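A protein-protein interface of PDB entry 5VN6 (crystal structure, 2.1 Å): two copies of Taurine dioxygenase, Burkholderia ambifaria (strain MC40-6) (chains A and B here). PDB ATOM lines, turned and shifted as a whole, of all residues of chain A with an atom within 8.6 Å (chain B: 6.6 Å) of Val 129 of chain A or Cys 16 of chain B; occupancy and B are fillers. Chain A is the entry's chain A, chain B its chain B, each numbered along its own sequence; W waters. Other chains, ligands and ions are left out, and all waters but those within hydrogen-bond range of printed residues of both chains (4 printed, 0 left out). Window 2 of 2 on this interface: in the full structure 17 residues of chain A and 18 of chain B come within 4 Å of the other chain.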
ATOM      1  N   GLY A 126      30.804 -26.004  26.099  1.00  0.00           N
ATOM      2  CA  GLY A 126      30.424 -24.614  26.061  1.00  0.00           C
ATOM      3  C   GLY A 126      30.896 -23.836  27.271  1.00  0.00           C
ATOM      4  O   GLY A 126      31.488 -24.384  28.205  1.00  0.00           O
ATOM      5  N   PRO A 127      30.622 -22.530  27.280  1.00  0.00           N
ATOM      6  CA  PRO A 127      31.063 -21.702  28.401  1.00  0.00           C
ATOM      7  C   PRO A 127      30.213 -21.945  29.630  1.00  0.00           C
ATOM      8  O   PRO A 127      29.047 -22.374  29.529  1.00  0.00           O
ATOM      9  CB  PRO A 127      30.885 -20.268  27.866  1.00  0.00           C
ATOM     10  CG  PRO A 127      29.745 -20.385  26.900  1.00  0.00           C
ATOM     11  CD  PRO A 127      29.830 -21.773  26.295  1.00  0.00           C
ATOM     12  N   PRO A 128      30.755 -21.699  30.828  1.00  0.00           N
ATOM     13  CA  PRO A 128      29.979 -21.956  32.051  1.00  0.00           C
ATOM     14  C   PRO A 128      28.786 -21.037  32.208  1.00  0.00           C
ATOM     15  O   PRO A 128      27.812 -21.405  32.879  1.00  0.00           O
ATOM     16  CB  PRO A 128      31.006 -21.734  33.170  1.00  0.00           C
ATOM     17  CG  PRO A 128      32.030 -20.813  32.562  1.00  0.00           C
ATOM     18  CD  PRO A 128      32.113 -21.201  31.121  1.00  0.00           C
ATOM     19  N   VAL A 129      28.838 -19.843  31.626  1.00  0.00           N
ATOM     20  CA  VAL A 129      27.738 -18.893  31.686  1.00  0.00           C
ATOM     21  C   VAL A 129      27.443 -18.392  30.280  1.00  0.00           C
ATOM     22  O   VAL A 129      28.343 -18.257  29.445  1.00  0.00           O
ATOM     23  CB  VAL A 129      28.049 -17.704  32.634  1.00  0.00           C
ATOM     24  CG1 VAL A 129      28.541 -18.208  33.989  1.00  0.00           C
ATOM     25  CG2 VAL A 129      29.086 -16.770  32.015  1.00  0.00           C
ATOM     26  N   GLY A 130      26.170 -18.128  30.020  1.00  0.00           N
ATOM     27  CA  GLY A 130      25.746 -17.519  28.776  1.00  0.00           C
ATOM     28  C   GLY A 130      25.185 -18.535  27.792  1.00  0.00           C
ATOM     29  O   GLY A 130      25.378 -19.749  27.918  1.00  0.00           O
ATOM     30  N   GLY A 131      24.473 -18.018  26.791  1.00  0.00           N
ATOM     31  CA  GLY A 131      23.965 -18.867  25.728  1.00  0.00           C
ATOM     32  C   GLY A 131      22.732 -19.683  26.055  1.00  0.00           C
ATOM     33  O   GLY A 131      22.542 -20.759  25.471  1.00  0.00           O
ATOM     34  N   ASP A 132      21.889 -19.207  26.975  1.00  0.00           N
ATOM     35  CA  ASP A 132      20.624 -19.873  27.271  1.00  0.00           C
ATOM     36  C   ASP A 132      19.750 -19.958  26.020  1.00  0.00           C
ATOM     37  O   ASP A 132      19.882 -19.169  25.087  1.00  0.00           O
ATOM     38  CB  ASP A 132      19.854 -19.103  28.346  1.00  0.00           C
ATOM     39  CG  ASP A 132      20.497 -19.190  29.704  1.00  0.00           C
ATOM     40  OD1 ASP A 132      21.563 -19.832  29.824  1.00  0.00           O
ATOM     41  OD2 ASP A 132      19.945 -18.582  30.647  1.00  0.00           O
ATOM     42  N   ARG A 248      13.032 -20.644  30.057  1.00  0.00           N
ATOM     43  CA  ARG A 248      14.429 -20.334  29.773  1.00  0.00           C
ATOM     44  C   ARG A 248      15.306 -21.443  30.328  1.00  0.00           C
ATOM     45  O   ARG A 248      15.198 -21.788  31.502  1.00  0.00           O
ATOM     46  CB  ARG A 248      14.847 -18.980  30.367  1.00  0.00           C
ATOM     47  CG  ARG A 248      16.319 -18.636  30.098  1.00  0.00           C
ATOM     48  CD  ARG A 248      16.542 -17.138  29.992  1.00  0.00           C
ATOM     49  NE  ARG A 248      17.952 -16.795  29.817  1.00  0.00           N
ATOM     50  CZ  ARG A 248      18.391 -15.603  29.409  1.00  0.00           C
ATOM     51  NH1 ARG A 248      19.692 -15.380  29.271  1.00  0.00           N
ATOM     52  NH2 ARG A 248      17.532 -14.639  29.121  1.00  0.00           N
ATOM     53  N   ARG A 250      19.161 -23.212  30.832  1.00  0.00           N
ATOM     54  CA  ARG A 250      20.597 -22.987  30.914  1.00  0.00           C
ATOM     55  C   ARG A 250      21.320 -24.282  30.597  1.00  0.00           C
ATOM     56  O   ARG A 250      21.041 -25.315  31.212  1.00  0.00           O
ATOM     57  CB  ARG A 250      21.005 -22.491  32.296  1.00  0.00           C
ATOM     58  CG  ARG A 250      22.477 -22.187  32.364  1.00  0.00           C
ATOM     59  CD  ARG A 250      22.829 -21.483  33.664  1.00  0.00           C
ATOM     60  NE  ARG A 250      24.265 -21.322  33.783  1.00  0.00           N
ATOM     61  CZ  ARG A 250      24.869 -20.723  34.805  1.00  0.00           C
ATOM     62  NH1 ARG A 250      24.152 -20.219  35.807  1.00  0.00           N
ATOM     63  NH2 ARG A 250      26.190 -20.626  34.814  1.00  0.00           N
ATOM     64  N   TRP A 251      22.230 -24.228  29.631  1.00  0.00           N
ATOM     65  CA  TRP A 251      22.908 -25.429  29.147  1.00  0.00           C
ATOM     66  C   TRP A 251      24.060 -25.842  30.055  1.00  0.00           C
ATOM     67  O   TRP A 251      24.757 -25.004  30.636  1.00  0.00           O
ATOM     68  CB  TRP A 251      23.444 -25.208  27.733  1.00  0.00           C
ATOM     69  CG  TRP A 251      22.358 -25.004  26.734  1.00  0.00           C
ATOM     70  CD1 TRP A 251      21.862 -23.812  26.274  1.00  0.00           C
ATOM     71  CD2 TRP A 251      21.587 -26.036  26.102  1.00  0.00           C
ATOM     72  NE1 TRP A 251      20.831 -24.047  25.374  1.00  0.00           N
ATOM     73  CE2 TRP A 251      20.649 -25.404  25.256  1.00  0.00           C
ATOM     74  CE3 TRP A 251      21.610 -27.432  26.163  1.00  0.00           C
ATOM     75  CZ2 TRP A 251      19.751 -26.124  24.467  1.00  0.00           C
ATOM     76  CZ3 TRP A 251      20.699 -28.146  25.395  1.00  0.00           C
ATOM     77  CH2 TRP A 251      19.785 -27.488  24.556  1.00  0.00           C
ATOM     78  N   LYS A 252      24.259 -27.154  30.158  1.00  0.00           N
ATOM     79  CA  LYS A 252      25.438 -27.772  30.755  1.00  0.00           C
ATOM     80  C   LYS A 252      25.933 -28.847  29.799  1.00  0.00           C
ATOM     81  O   LYS A 252      25.230 -29.237  28.864  1.00  0.00           O
ATOM     82  CB  LYS A 252      25.122 -28.392  32.124  1.00  0.00           C
ATOM     83  CG  LYS A 252      24.579 -27.404  33.168  1.00  0.00           C
ATOM     84  CD  LYS A 252      25.663 -26.500  33.689  1.00  0.00           C
ATOM     85  CE  LYS A 252      25.087 -25.363  34.528  1.00  0.00           C
ATOM     86  NZ  LYS A 252      26.143 -24.362  34.826  1.00  0.00           N
ATOM     87  N   VAL A 269      19.658 -17.231  22.991  1.00  0.00           N
ATOM     88  CA  VAL A 269      20.105 -15.947  23.525  1.00  0.00           C
ATOM     89  C   VAL A 269      21.566 -15.698  23.176  1.00  0.00           C
ATOM     90  O   VAL A 269      22.446 -16.531  23.431  1.00  0.00           O
ATOM     91  CB  VAL A 269      19.873 -15.876  25.040  1.00  0.00           C
ATOM     92  CG1 VAL A 269      20.201 -14.492  25.531  1.00  0.00           C
ATOM     93  CG2 VAL A 269      18.413 -16.214  25.369  1.00  0.00           C
ATOM     94  N   MET A 270      21.846 -14.514  22.645  1.00  0.00           N
ATOM     95  CA  MET A 270      23.202 -14.216  22.224  1.00  0.00           C
ATOM     96  C   MET A 270      23.827 -13.174  23.149  1.00  0.00           C
ATOM     97  O   MET A 270      24.207 -12.091  22.696  1.00  0.00           O
ATOM     98  CB  MET A 270      23.208 -13.719  20.782  1.00  0.00           C
ATOM     99  CG  MET A 270      24.377 -14.229  19.975  1.00  0.00           C
ATOM    100  SD  MET A 270      24.009 -15.898  19.430  1.00  0.00           S
ATOM    101  CE  MET A 270      22.626 -15.574  18.338  1.00  0.00           C
ATOM    102  N   ASP A 271      23.922 -13.491  24.441  1.00  0.00           N
ATOM    103  CA  ASP A 271      24.517 -12.607  25.432  1.00  0.00           C
ATOM    104  C   ASP A 271      26.014 -12.803  25.587  1.00  0.00           C
ATOM    105  O   ASP A 271      26.636 -12.065  26.360  1.00  0.00           O
ATOM    106  CB  ASP A 271      23.844 -12.797  26.805  1.00  0.00           C
ATOM    107  CG  ASP A 271      23.928 -14.233  27.309  1.00  0.00           C
ATOM    108  OD1 ASP A 271      24.026 -15.150  26.465  1.00  0.00           O
ATOM    109  OD2 ASP A 271      23.882 -14.454  28.538  1.00  0.00           O
ATOM    110  N   TYR A 272      26.642 -13.788  24.813  1.00  0.00           N
ATOM    111  CA  TYR A 272      28.016 -14.151  25.126  1.00  0.00           C
ATOM    112  C   TYR A 272      29.002 -13.559  24.126  1.00  0.00           C
ATOM    113  O   TYR A 272      28.678 -13.374  22.948  1.00  0.00           O
ATOM    114  CB  TYR A 272      28.205 -15.676  25.172  1.00  0.00           C
ATOM    115  CG  TYR A 272      27.658 -16.475  23.997  1.00  0.00           C
ATOM    116  CD1 TYR A 272      28.491 -16.870  22.955  1.00  0.00           C
ATOM    117  CD2 TYR A 272      26.323 -16.865  23.946  1.00  0.00           C
ATOM    118  CE1 TYR A 272      28.006 -17.612  21.885  1.00  0.00           C
ATOM    119  CE2 TYR A 272      25.830 -17.612  22.879  1.00  0.00           C
ATOM    120  CZ  TYR A 272      26.679 -17.979  21.851  1.00  0.00           C
ATOM    121  OH  TYR A 272      26.207 -18.718  20.787  1.00  0.00           O
ATOM    122  N   PRO A 273      30.200 -13.244  24.617  1.00  0.00           N
ATOM    123  CA  PRO A 273      31.304 -12.818  23.744  1.00  0.00           C
ATOM    124  C   PRO A 273      31.791 -13.969  22.880  1.00  0.00           C
ATOM    125  O   PRO A 273      31.351 -15.116  23.064  1.00  0.00           O
ATOM    126  CB  PRO A 273      32.389 -12.374  24.743  1.00  0.00           C
ATOM    127  CG  PRO A 273      31.680 -12.173  26.043  1.00  0.00           C
ATOM    128  CD  PRO A 273      30.561 -13.166  26.043  1.00  0.00           C
ATOM    129  N   CYS A 275      33.294 -17.116  21.761  1.00  0.00           N
ATOM    130  CA  CYS A 275      33.762 -18.255  22.532  1.00  0.00           C
ATOM    131  C   CYS A 275      33.501 -19.527  21.739  1.00  0.00           C
ATOM    132  O   CYS A 275      32.890 -19.503  20.666  1.00  0.00           O
ATOM    133  CB  CYS A 275      33.071 -18.314  23.897  1.00  0.00           C
ATOM    134  SG  CYS A 275      31.333 -18.796  23.788  1.00  0.00           S
ATOM    135  N   ARG A 277      31.568 -22.878  21.541  1.00  0.00           N
ATOM    136  CA  ARG A 277      30.413 -23.632  21.993  1.00  0.00           C
ATOM    137  C   ARG A 277      30.092 -24.656  20.921  1.00  0.00           C
ATOM    138  O   ARG A 277      30.026 -24.313  19.736  1.00  0.00           O
ATOM    139  CB  ARG A 277      29.209 -22.733  22.230  1.00  0.00           C
ATOM    140  CG  ARG A 277      28.122 -23.385  23.046  1.00  0.00           C
ATOM    141  CD  ARG A 277      27.074 -22.373  23.411  1.00  0.00           C
ATOM    142  NE  ARG A 277      26.116 -22.201  22.323  1.00  0.00           N
ATOM    143  CZ  ARG A 277      24.800 -22.098  22.486  1.00  0.00           C
ATOM    144  NH1 ARG A 277      24.268 -22.152  23.701  1.00  0.00           N
ATOM    145  NH2 ARG A 277      24.012 -21.952  21.431  1.00  0.00           N
ATOM    146  N   GLU B  12      28.185 -16.708  41.431  1.00  0.00           N
ATOM    147  CA  GLU B  12      27.937 -17.496  40.217  1.00  0.00           C
ATOM    148  C   GLU B  12      26.935 -16.765  39.339  1.00  0.00           C
ATOM    149  O   GLU B  12      25.719 -16.850  39.588  1.00  0.00           O
ATOM    150  CB  GLU B  12      27.422 -18.889  40.575  1.00  0.00           C
ATOM    151  N   PRO B  13      27.382 -16.011  38.329  1.00  0.00           N
ATOM    152  CA  PRO B  13      26.430 -15.303  37.461  1.00  0.00           C
ATOM    153  C   PRO B  13      25.497 -16.268  36.741  1.00  0.00           C
ATOM    154  O   PRO B  13      25.888 -17.374  36.357  1.00  0.00           O
ATOM    155  CB  PRO B  13      27.329 -14.547  36.473  1.00  0.00           C
ATOM    156  CG  PRO B  13      28.697 -15.149  36.619  1.00  0.00           C
ATOM    157  CD  PRO B  13      28.781 -15.686  38.007  1.00  0.00           C
ATOM    158  N   LEU B  14      24.252 -15.836  36.558  1.00  0.00           N
ATOM    159  CA  LEU B  14      23.262 -16.668  35.881  1.00  0.00           C
ATOM    160  C   LEU B  14      23.287 -16.493  34.370  1.00  0.00           C
ATOM    161  O   LEU B  14      23.004 -17.451  33.640  1.00  0.00           O
ATOM    162  CB  LEU B  14      21.860 -16.368  36.418  1.00  0.00           C
ATOM    163  CG  LEU B  14      21.496 -17.086  37.715  1.00  0.00           C
ATOM    164  CD1 LEU B  14      22.328 -16.558  38.863  1.00  0.00           C
ATOM    165  CD2 LEU B  14      20.023 -16.881  38.014  1.00  0.00           C
ATOM    166  N   THR B  15      23.633 -15.298  33.898  1.00  0.00           N
ATOM    167  CA  THR B  15      23.734 -14.948  32.488  1.00  0.00           C
ATOM    168  C   THR B  15      24.956 -14.052  32.328  1.00  0.00           C
ATOM    169  O   THR B  15      25.599 -13.663  33.309  1.00  0.00           O
ATOM    170  CB  THR B  15      22.484 -14.209  31.975  1.00  0.00           C
ATOM    171  OG1 THR B  15      22.453 -12.880  32.525  1.00  0.00           O
ATOM    172  CG2 THR B  15      21.203 -14.927  32.355  1.00  0.00           C
ATOM    173  N   CYS B  16      25.298 -13.734  31.080  1.00  0.00           N
ATOM    174  CA  CYS B  16      26.403 -12.801  30.870  1.00  0.00           C
ATOM    175  C   CYS B  16      25.990 -11.358  31.093  1.00  0.00           C
ATOM    176  O   CYS B  16      26.862 -10.486  31.214  1.00  0.00           O
ATOM    177  CB  CYS B  16      26.975 -12.940  29.458  1.00  0.00           C
ATOM    178  SG  CYS B  16      27.780 -14.519  29.109  1.00  0.00           S
ATOM    179  N   ALA B  17      24.689 -11.085  31.143  1.00  0.00           N
ATOM    180  CA  ALA B  17      24.180  -9.724  31.217  1.00  0.00           C
ATOM    181  C   ALA B  17      23.789  -9.309  32.623  1.00  0.00           C
ATOM    182  O   ALA B  17      23.965  -8.146  32.978  1.00  0.00           O
ATOM    183  CB  ALA B  17      22.954  -9.558  30.309  1.00  0.00           C
ATOM    184  N   ILE B  18      23.263 -10.231  33.432  1.00  0.00           N
ATOM    185  CA  ILE B  18      22.583  -9.825  34.654  1.00  0.00           C
ATOM    186  C   ILE B  18      22.341 -11.009  35.583  1.00  0.00           C
ATOM    187  O   ILE B  18      21.996 -12.120  35.148  1.00  0.00           O
ATOM    188  CB  ILE B  18      21.266  -9.098  34.312  1.00  0.00           C
ATOM    189  CG1 ILE B  18      20.553  -8.624  35.581  1.00  0.00           C
ATOM    190  CG2 ILE B  18      20.350  -9.998  33.462  1.00  0.00           C
ATOM    191  CD1 ILE B  18      19.450  -7.598  35.320  1.00  0.00           C
ATOM    192  N   GLY B  19      22.515 -10.774  36.878  1.00  0.00           N
ATOM    193  CA  GLY B  19      22.142 -11.756  37.867  1.00  0.00           C
ATOM    194  C   GLY B  19      23.303 -12.616  38.286  1.00  0.00           C
ATOM    195  O   GLY B  19      24.129 -13.011  37.456  1.00  0.00           O
ATOM    196  N   ASN B 137      18.356  -5.741  32.495  1.00  0.00           N
ATOM    197  CA  ASN B 137      19.476  -4.817  32.703  1.00  0.00           C
ATOM    198  C   ASN B 137      19.254  -3.606  31.800  1.00  0.00           C
ATOM    199  O   ASN B 137      19.515  -3.661  30.595  1.00  0.00           O
ATOM    200  CB  ASN B 137      20.783  -5.539  32.400  1.00  0.00           C
ATOM    201  CG  ASN B 137      22.018  -4.662  32.522  1.00  0.00           C
ATOM    202  OD1 ASN B 137      21.958  -3.438  32.428  1.00  0.00           O
ATOM    203  ND2 ASN B 137      23.166  -5.315  32.700  1.00  0.00           N
ATOM    204  N   LEU B 140      22.583  -1.995  30.101  1.00  0.00           N
ATOM    205  CA  LEU B 140      22.875  -2.626  28.825  1.00  0.00           C
ATOM    206  C   LEU B 140      21.846  -2.215  27.776  1.00  0.00           C
ATOM    207  O   LEU B 140      22.194  -1.983  26.610  1.00  0.00           O
ATOM    208  CB  LEU B 140      22.910  -4.142  29.009  1.00  0.00           C
ATOM    209  CG  LEU B 140      23.625  -4.983  27.956  1.00  0.00           C
ATOM    210  CD1 LEU B 140      25.040  -4.438  27.766  1.00  0.00           C
ATOM    211  CD2 LEU B 140      23.648  -6.445  28.390  1.00  0.00           C
ATOM    212  N   GLU B 244      18.353 -11.007  25.616  1.00  0.00           N
ATOM    213  CA  GLU B 244      19.764 -10.767  25.882  1.00  0.00           C
ATOM    214  C   GLU B 244      19.983  -9.971  27.161  1.00  0.00           C
ATOM    215  O   GLU B 244      21.058 -10.056  27.765  1.00  0.00           O
ATOM    216  CB  GLU B 244      20.393 -10.036  24.694  1.00  0.00           C
ATOM    217  CG  GLU B 244      20.937 -10.945  23.616  1.00  0.00           C
ATOM    218  CD  GLU B 244      19.850 -11.535  22.688  1.00  0.00           C
ATOM    219  OE1 GLU B 244      20.230 -12.359  21.831  1.00  0.00           O
ATOM    220  OE2 GLU B 244      18.637 -11.163  22.775  1.00  0.00           O
HETATM  221  O   HOH W   1      23.410 -18.518  31.234  1.00  0.00           O
HETATM  222  O   HOH W   2      20.635 -12.510  29.355  1.00  0.00           O
HETATM  223  O   HOH W   3      24.624 -19.274  38.338  1.00  0.00           O
HETATM  224  O   HOH W   4      20.017 -18.249  33.221  1.00  0.00           O
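NE of Arg 248 of chain A lies within salt-bridge range of OD2 of Asp 132 of chain A, at 2.8 Å. OG1 of Thr 15 of chain B is in hydrogen-bond range of O of Ile 18 of chain B (2.8 Å). The backbone NH (N) of Leu 14 of chain B is in hydrogen-bond range of the backbone carbonyl oxygen (O) of Gly 19 of chain B (3.0 Å). The backbone carbonyl oxygen (O) of Pro 128 of chain A is in hydrogen-bond range of the guanidinium group (NH2) of Arg 250 of chain A, at 2.6 Å. The backbone NH (N) of Val 269 of chain A sits at hydrogen-bond distance from the backbone carbonyl oxygen (O) of Asp 132 of chain A (2.9 Å). N of Gly 131 of chain A is in hydrogen-bond range of OD1 of Asp 271 of chain A (2.9 Å).
Of the 18 printed residues of chain A, 7 touch a printed residue of chain B. Hydrophobic or aromatic side chains of chain A within 4 Å of the printed part of chain B: Val 129, Val 269 and Met 270. Of the 11 printed residues of chain B, 5 touch a printed residue of chain A.
Among the printed residues, pairs that only touch across the chains: Val 129 of chain A with Pro 13 of chain B, Gly 130 of chain A with Cys 16 of chain B, Arg 248 of chain A with Thr 15 of chain B, Arg 250 of chain A with Leu 14 of chain B, Val 269 of chain A with Glu 244 of chain B and Asp 271 of chain A with Thr 15 of chain B.
Water W4 lies within hydrogen-bond range of the side-chain carboxylate of Asp 132 of chain A (2.6 Å) and the backbone carbonyl oxygen of Leu 14 of chain B (3.1 Å). Water W1 lies within hydrogen-bond range of O of Leu 14 of chain B, OD1 of Asp 132 of chain A and N of Gly 130 of chain A. Water W3 lies within hydrogen-bond range of the guanidinium group of Arg 250 of chain A (2.7 Å), the backbone carbonyl oxygen of Glu 12 of chain B (2.9 Å) and the backbone carbonyl oxygen of Pro 13 of chain B (3.0 Å). Water W2 bridges the backbone carbonyl oxygen of Glu 244 of chain B (3.0 Å) and the guanidinium group of Arg 248 of chain A (3.0 Å).
The guanidinium group (NH1) of Arg 250 of chain A sits at hydrogen-bond distance from the backbone carbonyl oxygen (O) of Pro 13 of chain B (3.4 Å). N of Cys 16 of chain B is in hydrogen-bond range of OD2 of Asp 271 of chain A (3.0 Å). The backbone NH (N) of Met 270 of chain A lies within hydrogen-bond range of the side-chain carboxylate (OE1) of Glu 244 of chain B (2.8 Å). SG of Cys 16 of chain B lies within hydrogen-bond range of O of Val 129 of chain A.
No position is printed for both chains. Of the 10 pairs that touch across the chains among the printed residues, none has its exchanged pair printed and touching as well.
Of chain B, only Pro 13 (3.7 Å) and Cys 16 (3.8 Å) come within 4 Å of Val 129 of chain A. Printed residues of chain B within 4 Å of Gly 130 of chain A: Cys 16. Of the printed residues of chain B, Met 270 of chain A touches Glu 244. Printed residues of chain A within 4 Å of Leu 14 of chain B: Arg 250 (3.7 Å). Of the printed residues of chain A, Cys 16 of chain B touches Val 129, Gly 130 and Asp 271. The nearest printed residue of chain A that does not touch Cys 16 of chain B is Tyr 272 of chain A (4.01 Å). The nearest printed residue of chain A that does not touch Glu 244 of chain B is Asp 271 of chain A (4.01 Å).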
